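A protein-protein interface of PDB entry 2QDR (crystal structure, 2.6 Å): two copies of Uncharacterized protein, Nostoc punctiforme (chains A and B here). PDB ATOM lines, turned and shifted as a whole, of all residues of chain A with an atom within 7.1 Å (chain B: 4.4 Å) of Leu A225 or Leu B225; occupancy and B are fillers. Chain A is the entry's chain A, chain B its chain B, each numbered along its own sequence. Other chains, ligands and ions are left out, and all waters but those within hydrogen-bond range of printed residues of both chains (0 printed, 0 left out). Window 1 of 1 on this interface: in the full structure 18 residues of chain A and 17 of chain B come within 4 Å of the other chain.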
ATOM      1  N   TRP A 194      27.567 -32.721  14.999  1.00  0.00           N
ATOM      2  CA  TRP A 194      27.111 -31.354  15.289  1.00  0.00           C
ATOM      3  C   TRP A 194      28.287 -30.396  15.361  1.00  0.00           C
ATOM      4  O   TRP A 194      29.341 -30.739  15.894  1.00  0.00           O
ATOM      5  CB  TRP A 194      26.323 -31.248  16.597  1.00  0.00           C
ATOM      6  CG  TRP A 194      24.985 -31.879  16.544  1.00  0.00           C
ATOM      7  CD1 TRP A 194      24.610 -33.042  17.120  1.00  0.00           C
ATOM      8  CD2 TRP A 194      23.836 -31.380  15.845  1.00  0.00           C
ATOM      9  NE1 TRP A 194      23.294 -33.292  16.851  1.00  0.00           N
ATOM     10  CE2 TRP A 194      22.790 -32.294  16.065  1.00  0.00           C
ATOM     11  CE3 TRP A 194      23.590 -30.248  15.056  1.00  0.00           C
ATOM     12  CZ2 TRP A 194      21.520 -32.129  15.508  1.00  0.00           C
ATOM     13  CZ3 TRP A 194      22.326 -30.087  14.487  1.00  0.00           C
ATOM     14  CH2 TRP A 194      21.309 -31.015  14.721  1.00  0.00           C
ATOM     15  N   GLY A 195      28.078 -29.194  14.832  1.00  0.00           N
ATOM     16  CA  GLY A 195      29.087 -28.140  14.820  1.00  0.00           C
ATOM     17  C   GLY A 195      28.497 -26.848  15.343  1.00  0.00           C
ATOM     18  O   GLY A 195      27.286 -26.768  15.617  1.00  0.00           O
ATOM     19  N   VAL A 203      23.733 -18.961  19.726  1.00  0.00           N
ATOM     20  CA  VAL A 203      25.004 -19.495  20.269  1.00  0.00           C
ATOM     21  C   VAL A 203      24.770 -20.818  21.044  1.00  0.00           C
ATOM     22  O   VAL A 203      25.586 -21.737  20.952  1.00  0.00           O
ATOM     23  CB  VAL A 203      25.784 -18.421  21.162  1.00  0.00           C
ATOM     24  CG1 VAL A 203      26.868 -19.041  22.083  1.00  0.00           C
ATOM     25  CG2 VAL A 203      26.390 -17.334  20.296  1.00  0.00           C
ATOM     26  N   GLN A 204      23.649 -20.906  21.776  1.00  0.00           N
ATOM     27  CA  GLN A 204      23.265 -22.094  22.555  1.00  0.00           C
ATOM     28  C   GLN A 204      22.420 -23.015  21.690  1.00  0.00           C
ATOM     29  O   GLN A 204      21.253 -23.308  21.978  1.00  0.00           O
ATOM     30  CB  GLN A 204      22.512 -21.694  23.832  1.00  0.00           C
ATOM     31  CG  GLN A 204      23.260 -20.804  24.840  1.00  0.00           C
ATOM     32  CD  GLN A 204      24.526 -21.435  25.434  1.00  0.00           C
ATOM     33  OE1 GLN A 204      24.595 -21.662  26.642  1.00  0.00           O
ATOM     34  NE2 GLN A 204      25.514 -21.741  24.591  1.00  0.00           N
ATOM     35  N   ALA A 205      23.050 -23.479  20.623  1.00  0.00           N
ATOM     36  CA  ALA A 205      22.442 -24.354  19.656  1.00  0.00           C
ATOM     37  C   ALA A 205      23.566 -24.856  18.794  1.00  0.00           C
ATOM     38  O   ALA A 205      24.678 -24.336  18.859  1.00  0.00           O
ATOM     39  CB  ALA A 205      21.432 -23.617  18.824  1.00  0.00           C
ATOM     40  N   ASN A 206      23.278 -25.891  18.024  1.00  0.00           N
ATOM     41  CA  ASN A 206      24.235 -26.482  17.116  1.00  0.00           C
ATOM     42  C   ASN A 206      23.604 -26.601  15.752  1.00  0.00           C
ATOM     43  O   ASN A 206      22.377 -26.646  15.629  1.00  0.00           O
ATOM     44  CB  ASN A 206      24.714 -27.826  17.647  1.00  0.00           C
ATOM     45  CG  ASN A 206      25.666 -27.683  18.820  1.00  0.00           C
ATOM     46  OD1 ASN A 206      25.494 -28.326  19.845  1.00  0.00           O
ATOM     47  ND2 ASN A 206      26.660 -26.814  18.683  1.00  0.00           N
ATOM     48  N   ALA A 223      19.796 -27.757  15.984  1.00  0.00           N
ATOM     49  CA  ALA A 223      19.501 -28.431  17.233  1.00  0.00           C
ATOM     50  C   ALA A 223      19.505 -27.349  18.283  1.00  0.00           C
ATOM     51  O   ALA A 223      20.557 -26.738  18.519  1.00  0.00           O
ATOM     52  CB  ALA A 223      20.530 -29.481  17.559  1.00  0.00           C
ATOM     53  N   ILE A 224      18.339 -27.078  18.873  1.00  0.00           N
ATOM     54  CA  ILE A 224      18.223 -26.073  19.921  1.00  0.00           C
ATOM     55  C   ILE A 224      18.277 -26.826  21.227  1.00  0.00           C
ATOM     56  O   ILE A 224      17.499 -27.759  21.433  1.00  0.00           O
ATOM     57  CB  ILE A 224      16.931 -25.254  19.849  1.00  0.00           C
ATOM     58  CG1 ILE A 224      16.856 -24.526  18.493  1.00  0.00           C
ATOM     59  CG2 ILE A 224      16.857 -24.271  21.055  1.00  0.00           C
ATOM     60  CD1 ILE A 224      15.637 -23.663  18.295  1.00  0.00           C
ATOM     61  N   LEU A 225      19.196 -26.430  22.100  1.00  0.00           N
ATOM     62  CA  LEU A 225      19.331 -27.082  23.390  1.00  0.00           C
ATOM     63  C   LEU A 225      18.203 -26.661  24.313  1.00  0.00           C
ATOM     64  O   LEU A 225      17.541 -25.656  24.045  1.00  0.00           O
ATOM     65  CB  LEU A 225      20.669 -26.713  24.041  1.00  0.00           C
ATOM     66  CG  LEU A 225      21.935 -27.139  23.292  1.00  0.00           C
ATOM     67  CD1 LEU A 225      23.206 -26.652  23.990  1.00  0.00           C
ATOM     68  CD2 LEU A 225      21.961 -28.624  23.155  1.00  0.00           C
ATOM     69  N   PRO A 226      17.953 -27.431  25.393  1.00  0.00           N
ATOM     70  CA  PRO A 226      16.920 -27.030  26.358  1.00  0.00           C
ATOM     71  C   PRO A 226      17.211 -25.663  27.013  1.00  0.00           C
ATOM     72  O   PRO A 226      18.274 -25.096  26.813  1.00  0.00           O
ATOM     73  CB  PRO A 226      16.983 -28.139  27.413  1.00  0.00           C
ATOM     74  CG  PRO A 226      17.568 -29.291  26.730  1.00  0.00           C
ATOM     75  CD  PRO A 226      18.551 -28.730  25.764  1.00  0.00           C
ATOM     76  N   HIS A 227      16.266 -25.147  27.786  1.00  0.00           N
ATOM     77  CA  HIS A 227      16.385 -23.837  28.458  1.00  0.00           C
ATOM     78  C   HIS A 227      16.868 -22.695  27.534  1.00  0.00           C
ATOM     79  O   HIS A 227      17.667 -21.854  27.951  1.00  0.00           O
ATOM     80  CB  HIS A 227      17.307 -23.887  29.698  1.00  0.00           C
ATOM     81  CG  HIS A 227      16.970 -24.966  30.672  1.00  0.00           C
ATOM     82  ND1 HIS A 227      17.928 -25.614  31.421  1.00  0.00           N
ATOM     83  CD2 HIS A 227      15.797 -25.576  30.955  1.00  0.00           C
ATOM     84  CE1 HIS A 227      17.349 -26.524  32.181  1.00  0.00           C
ATOM     85  NE2 HIS A 227      16.056 -26.523  31.917  1.00  0.00           N
ATOM     86  N   PHE A 228      16.378 -22.682  26.300  1.00  0.00           N
ATOM     87  CA  PHE A 228      16.757 -21.685  25.306  1.00  0.00           C
ATOM     88  C   PHE A 228      15.865 -20.463  25.393  1.00  0.00           C
ATOM     89  O   PHE A 228      14.665 -20.587  25.638  1.00  0.00           O
ATOM     90  CB  PHE A 228      16.684 -22.301  23.895  1.00  0.00           C
ATOM     91  CG  PHE A 228      16.998 -21.332  22.764  1.00  0.00           C
ATOM     92  CD1 PHE A 228      18.311 -21.009  22.446  1.00  0.00           C
ATOM     93  CD2 PHE A 228      15.973 -20.780  21.991  1.00  0.00           C
ATOM     94  CE1 PHE A 228      18.594 -20.135  21.400  1.00  0.00           C
ATOM     95  CE2 PHE A 228      16.247 -19.904  20.933  1.00  0.00           C
ATOM     96  CZ  PHE A 228      17.551 -19.584  20.635  1.00  0.00           C
ATOM     97  N   ASP A 229      16.472 -19.289  25.194  1.00  0.00           N
ATOM     98  CA  ASP A 229      15.776 -18.016  25.202  1.00  0.00           C
ATOM     99  C   ASP A 229      16.621 -16.990  24.434  1.00  0.00           C
ATOM    100  O   ASP A 229      17.594 -16.477  24.969  1.00  0.00           O
ATOM    101  CB  ASP A 229      15.503 -17.571  26.644  1.00  0.00           C
ATOM    102  CG  ASP A 229      14.640 -16.314  26.729  1.00  0.00           C
ATOM    103  OD1 ASP A 229      14.270 -15.751  25.687  1.00  0.00           O
ATOM    104  OD2 ASP A 229      14.309 -15.904  27.857  1.00  0.00           O
ATOM    105  N   THR A 275      12.133 -22.064  24.554  1.00  0.00           N
ATOM    106  CA  THR A 275      11.866 -23.505  24.634  1.00  0.00           C
ATOM    107  C   THR A 275      12.634 -24.133  25.794  1.00  0.00           C
ATOM    108  O   THR A 275      13.854 -24.040  25.862  1.00  0.00           O
ATOM    109  CB  THR A 275      12.159 -24.271  23.321  1.00  0.00           C
ATOM    110  OG1 THR A 275      12.100 -25.678  23.584  1.00  0.00           O
ATOM    111  CG2 THR A 275      13.518 -23.954  22.735  1.00  0.00           C
ATOM    112  N   ASP A 276      11.891 -24.730  26.721  1.00  0.00           N
ATOM    113  CA  ASP A 276      12.471 -25.386  27.881  1.00  0.00           C
ATOM    114  C   ASP A 276      12.951 -26.791  27.541  1.00  0.00           C
ATOM    115  O   ASP A 276      13.810 -27.310  28.236  1.00  0.00           O
ATOM    116  CB  ASP A 276      11.461 -25.449  29.031  1.00  0.00           C
ATOM    117  CG  ASP A 276      11.075 -24.075  29.565  1.00  0.00           C
ATOM    118  OD1 ASP A 276      11.864 -23.106  29.456  1.00  0.00           O
ATOM    119  OD2 ASP A 276       9.980 -23.977  30.141  1.00  0.00           O
ATOM    120  N   ASP A 277      12.402 -27.392  26.484  1.00  0.00           N
ATOM    121  CA  ASP A 277      12.750 -28.756  26.055  1.00  0.00           C
ATOM    122  C   ASP A 277      13.782 -28.834  24.934  1.00  0.00           C
ATOM    123  O   ASP A 277      14.535 -29.810  24.863  1.00  0.00           O
ATOM    124  CB  ASP A 277      11.476 -29.497  25.591  1.00  0.00           C
ATOM    125  CG  ASP A 277      10.457 -29.704  26.714  1.00  0.00           C
ATOM    126  OD1 ASP A 277      10.700 -29.282  27.869  1.00  0.00           O
ATOM    127  OD2 ASP A 277       9.382 -30.277  26.431  1.00  0.00           O
ATOM    128  N   GLY A 278      13.805 -27.834  24.052  1.00  0.00           N
ATOM    129  CA  GLY A 278      14.722 -27.816  22.923  1.00  0.00           C
ATOM    130  C   GLY A 278      14.054 -28.521  21.750  1.00  0.00           C
ATOM    131  O   GLY A 278      12.857 -28.824  21.813  1.00  0.00           O
ATOM    132  N   GLY A 279      14.809 -28.768  20.675  1.00  0.00           N
ATOM    133  CA  GLY A 279      14.258 -29.450  19.504  1.00  0.00           C
ATOM    134  C   GLY A 279      15.183 -29.539  18.306  1.00  0.00           C
ATOM    135  O   GLY A 279      16.278 -28.981  18.320  1.00  0.00           O
ATOM    136  N   TRP B 194      24.967 -23.482  28.789  1.00  0.00           N
ATOM    137  CA  TRP B 194      25.495 -24.807  28.478  1.00  0.00           C
ATOM    138  C   TRP B 194      26.982 -24.713  28.180  1.00  0.00           C
ATOM    139  O   TRP B 194      27.424 -23.762  27.537  1.00  0.00           O
ATOM    140  CB  TRP B 194      24.783 -25.448  27.279  1.00  0.00           C
ATOM    141  CG  TRP B 194      23.393 -25.857  27.567  1.00  0.00           C
ATOM    142  CD1 TRP B 194      22.261 -25.220  27.190  1.00  0.00           C
ATOM    143  CD2 TRP B 194      22.982 -27.001  28.332  1.00  0.00           C
ATOM    144  NE1 TRP B 194      21.163 -25.899  27.660  1.00  0.00           N
ATOM    145  CE2 TRP B 194      21.575 -26.997  28.363  1.00  0.00           C
ATOM    146  CE3 TRP B 194      23.667 -28.033  28.984  1.00  0.00           C
ATOM    147  CZ2 TRP B 194      20.834 -27.974  29.041  1.00  0.00           C
ATOM    148  CZ3 TRP B 194      22.927 -29.005  29.661  1.00  0.00           C
ATOM    149  CH2 TRP B 194      21.529 -28.962  29.687  1.00  0.00           C
ATOM    150  N   GLN B 204      29.251 -35.107  21.903  1.00  0.00           N
ATOM    151  CA  GLN B 204      28.057 -34.544  21.244  1.00  0.00           C
ATOM    152  C   GLN B 204      26.922 -34.384  22.267  1.00  0.00           C
ATOM    153  O   GLN B 204      25.823 -34.955  22.150  1.00  0.00           O
ATOM    154  CB  GLN B 204      27.618 -35.431  20.085  1.00  0.00           C
ATOM    155  CG  GLN B 204      28.627 -35.581  18.956  1.00  0.00           C
ATOM    156  CD  GLN B 204      28.881 -34.291  18.163  1.00  0.00           C
ATOM    157  OE1 GLN B 204      28.583 -33.183  18.605  1.00  0.00           O
ATOM    158  NE2 GLN B 204      29.456 -34.447  16.992  1.00  0.00           N
ATOM    159  N   ALA B 205      27.206 -33.549  23.254  1.00  0.00           N
ATOM    160  CA  ALA B 205      26.310 -33.272  24.335  1.00  0.00           C
ATOM    161  C   ALA B 205      26.896 -32.105  25.083  1.00  0.00           C
ATOM    162  O   ALA B 205      28.063 -31.768  24.896  1.00  0.00           O
ATOM    163  CB  ALA B 205      26.201 -34.486  25.258  1.00  0.00           C
ATOM    164  N   ASN B 206      26.081 -31.477  25.911  1.00  0.00           N
ATOM    165  CA  ASN B 206      26.539 -30.377  26.735  1.00  0.00           C
ATOM    166  C   ASN B 206      26.142 -30.654  28.167  1.00  0.00           C
ATOM    167  O   ASN B 206      25.246 -31.464  28.430  1.00  0.00           O
ATOM    168  CB  ASN B 206      26.077 -29.027  26.213  1.00  0.00           C
ATOM    169  CG  ASN B 206      26.799 -28.642  24.945  1.00  0.00           C
ATOM    170  OD1 ASN B 206      26.534 -29.181  23.877  1.00  0.00           O
ATOM    171  ND2 ASN B 206      27.703 -27.679  25.055  1.00  0.00           N
ATOM    172  N   ALA B 223      22.571 -32.384  28.501  1.00  0.00           N
ATOM    173  CA  ALA B 223      21.750 -32.154  27.322  1.00  0.00           C
ATOM    174  C   ALA B 223      22.357 -33.006  26.232  1.00  0.00           C
ATOM    175  O   ALA B 223      23.510 -32.784  25.856  1.00  0.00           O
ATOM    176  CB  ALA B 223      21.735 -30.700  26.901  1.00  0.00           C
ATOM    177  N   ILE B 224      21.612 -34.006  25.770  1.00  0.00           N
ATOM    178  CA  ILE B 224      22.066 -34.886  24.708  1.00  0.00           C
ATOM    179  C   ILE B 224      21.423 -34.349  23.457  1.00  0.00           C
ATOM    180  O   ILE B 224      20.202 -34.222  23.399  1.00  0.00           O
ATOM    181  CB  ILE B 224      21.672 -36.362  24.932  1.00  0.00           C
ATOM    182  CG1 ILE B 224      22.297 -36.873  26.223  1.00  0.00           C
ATOM    183  CG2 ILE B 224      22.114 -37.235  23.733  1.00  0.00           C
ATOM    184  CD1 ILE B 224      21.976 -38.328  26.561  1.00  0.00           C
ATOM    185  N   LEU B 225      22.245 -34.015  22.467  1.00  0.00           N
ATOM    186  CA  LEU B 225      21.759 -33.500  21.203  1.00  0.00           C
ATOM    187  C   LEU B 225      21.085 -34.606  20.414  1.00  0.00           C
ATOM    188  O   LEU B 225      21.302 -35.776  20.719  1.00  0.00           O
ATOM    189  CB  LEU B 225      22.933 -32.985  20.382  1.00  0.00           C
ATOM    190  CG  LEU B 225      23.661 -31.738  20.894  1.00  0.00           C
ATOM    191  CD1 LEU B 225      25.054 -31.565  20.290  1.00  0.00           C
ATOM    192  CD2 LEU B 225      22.824 -30.518  20.603  1.00  0.00           C
ATOM    193  N   PRO B 226      20.241 -34.257  19.420  1.00  0.00           N
ATOM    194  CA  PRO B 226      19.625 -35.288  18.565  1.00  0.00           C
ATOM    195  C   PRO B 226      20.667 -36.143  17.819  1.00  0.00           C
ATOM    196  O   PRO B 226      21.849 -35.848  17.880  1.00  0.00           O
ATOM    197  CB  PRO B 226      18.796 -34.464  17.566  1.00  0.00           C
ATOM    198  CG  PRO B 226      18.551 -33.170  18.243  1.00  0.00           C
ATOM    199  CD  PRO B 226      19.743 -32.906  19.091  1.00  0.00           C
ATOM    200  N   HIS B 227      20.221 -37.193  17.130  1.00  0.00           N
ATOM    201  CA  HIS B 227      21.098 -38.118  16.371  1.00  0.00           C
ATOM    202  C   HIS B 227      22.351 -38.587  17.142  1.00  0.00           C
ATOM    203  O   HIS B 227      23.440 -38.697  16.572  1.00  0.00           O
ATOM    204  CB  HIS B 227      21.544 -37.510  15.042  1.00  0.00           C
ATOM    205  CG  HIS B 227      20.426 -37.024  14.181  1.00  0.00           C
ATOM    206  ND1 HIS B 227      20.543 -35.919  13.369  1.00  0.00           N
ATOM    207  CD2 HIS B 227      19.148 -37.448  14.056  1.00  0.00           C
ATOM    208  CE1 HIS B 227      19.409 -35.731  12.721  1.00  0.00           C
ATOM    209  NE2 HIS B 227      18.542 -36.638  13.127  1.00  0.00           N
ATOM    210  N   PHE B 228      22.177 -38.865  18.429  1.00  0.00           N
ATOM    211  CA  PHE B 228      23.264 -39.304  19.287  1.00  0.00           C
ATOM    212  C   PHE B 228      23.418 -40.822  19.252  1.00  0.00           C
ATOM    213  O   PHE B 228      22.421 -41.551  19.163  1.00  0.00           O
ATOM    214  CB  PHE B 228      23.016 -38.809  20.723  1.00  0.00           C
ATOM    215  CG  PHE B 228      24.051 -39.250  21.738  1.00  0.00           C
ATOM    216  CD1 PHE B 228      25.292 -38.623  21.807  1.00  0.00           C
ATOM    217  CD2 PHE B 228      23.751 -40.236  22.686  1.00  0.00           C
ATOM    218  CE1 PHE B 228      26.248 -39.010  22.788  1.00  0.00           C
ATOM    219  CE2 PHE B 228      24.698 -40.625  23.679  1.00  0.00           C
ATOM    220  CZ  PHE B 228      25.944 -40.011  23.728  1.00  0.00           C
ATOM    221  N   GLY B 278      17.099 -36.731  21.250  1.00  0.00           N
ATOM    222  CA  GLY B 278      17.926 -36.084  22.261  1.00  0.00           C
ATOM    223  C   GLY B 278      17.131 -35.990  23.543  1.00  0.00           C
ATOM    224  O   GLY B 278      16.062 -36.596  23.656  1.00  0.00           O
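Leu B225 touches just these residues of chain A: Trp A194, Asn A206, Ala A223 and Leu A225. Printed residues of chain A within 4 Å of Ala B223: Pro A226. Of the printed residues of chain B, Pro A226 touches Trp B194 and Ala B223. The nearest printed residue of chain B that does not touch Pro A226 is Ile B224 (6.1 Å).
Printed residues of chain B that touch a printed residue of chain A: Trp B194, Gln B204, Ala B223, Leu B225 and Pro B226. Hydrophobic or aromatic side chains of chain B within 4 Å of the printed part of chain A: Trp B194, Ala B223, Leu B225 and Pro B226. Hydrophobic or aromatic side chains of chain A within 4 Å of the printed part of chain B: Trp A194, Ala A223, Leu A225 and Pro A226.
Trp A194 touches Gln B204, and with the chains exchanged Gln A204 touches Trp B194. Trp A194 touches Leu B225, and with the chains exchanged Leu A225 touches Trp B194. Trp A194 touches Pro B226, and with the chains exchanged Pro A226 touches Trp B194. Leu B225 touches its own counterpart, Leu A225. Positions printed for both chains: 194, 204, 205, 206, 223, 224, 225, 226, 227, 228 and 278.
The backbone carbonyl oxygen (O) of Asn A206 sits at hydrogen-bond distance from the backbone NH (N) of Ala A223. The backbone carbonyl oxygen of Gly A195 lies within hydrogen-bond range of the side-chain amide nitrogen of Asn A206. O of Asn B206 sits at hydrogen-bond distance from N of Ala B223, 2.8 Å away.
The backbone NH (N) of Trp A194 sits close to the side-chain amide nitrogen (NE2) of Gln B204 (3.2 Å). O of Pro B226 is in hydrogen-bond range of NE1 of Trp A194 (3.1 Å). The side-chain amide oxygen (OE1) of Gln A204 lies within hydrogen-bond range of the backbone NH (N) of Trp B194, at 2.8 Å. The backbone carbonyl oxygen (O) of Pro A226 sits at hydrogen-bond distance from the indole nitrogen (NE1) of Trp B194 (3.1 Å).
Among the printed residues, pairs that only touch across the chains: Trp A194 with Leu B225 (3.5 Å), Asn A206 with Leu B225 (3.3 Å), Ala A223 with Leu B225 (3.95 Å), Ala A223 with Pro B226 (3.8 Å), Leu A225 with Trp B194 (3.6 Å), Leu A225 with Leu B225 (3.3 Å) and Pro A226 with Ala B223 (3.9 Å).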
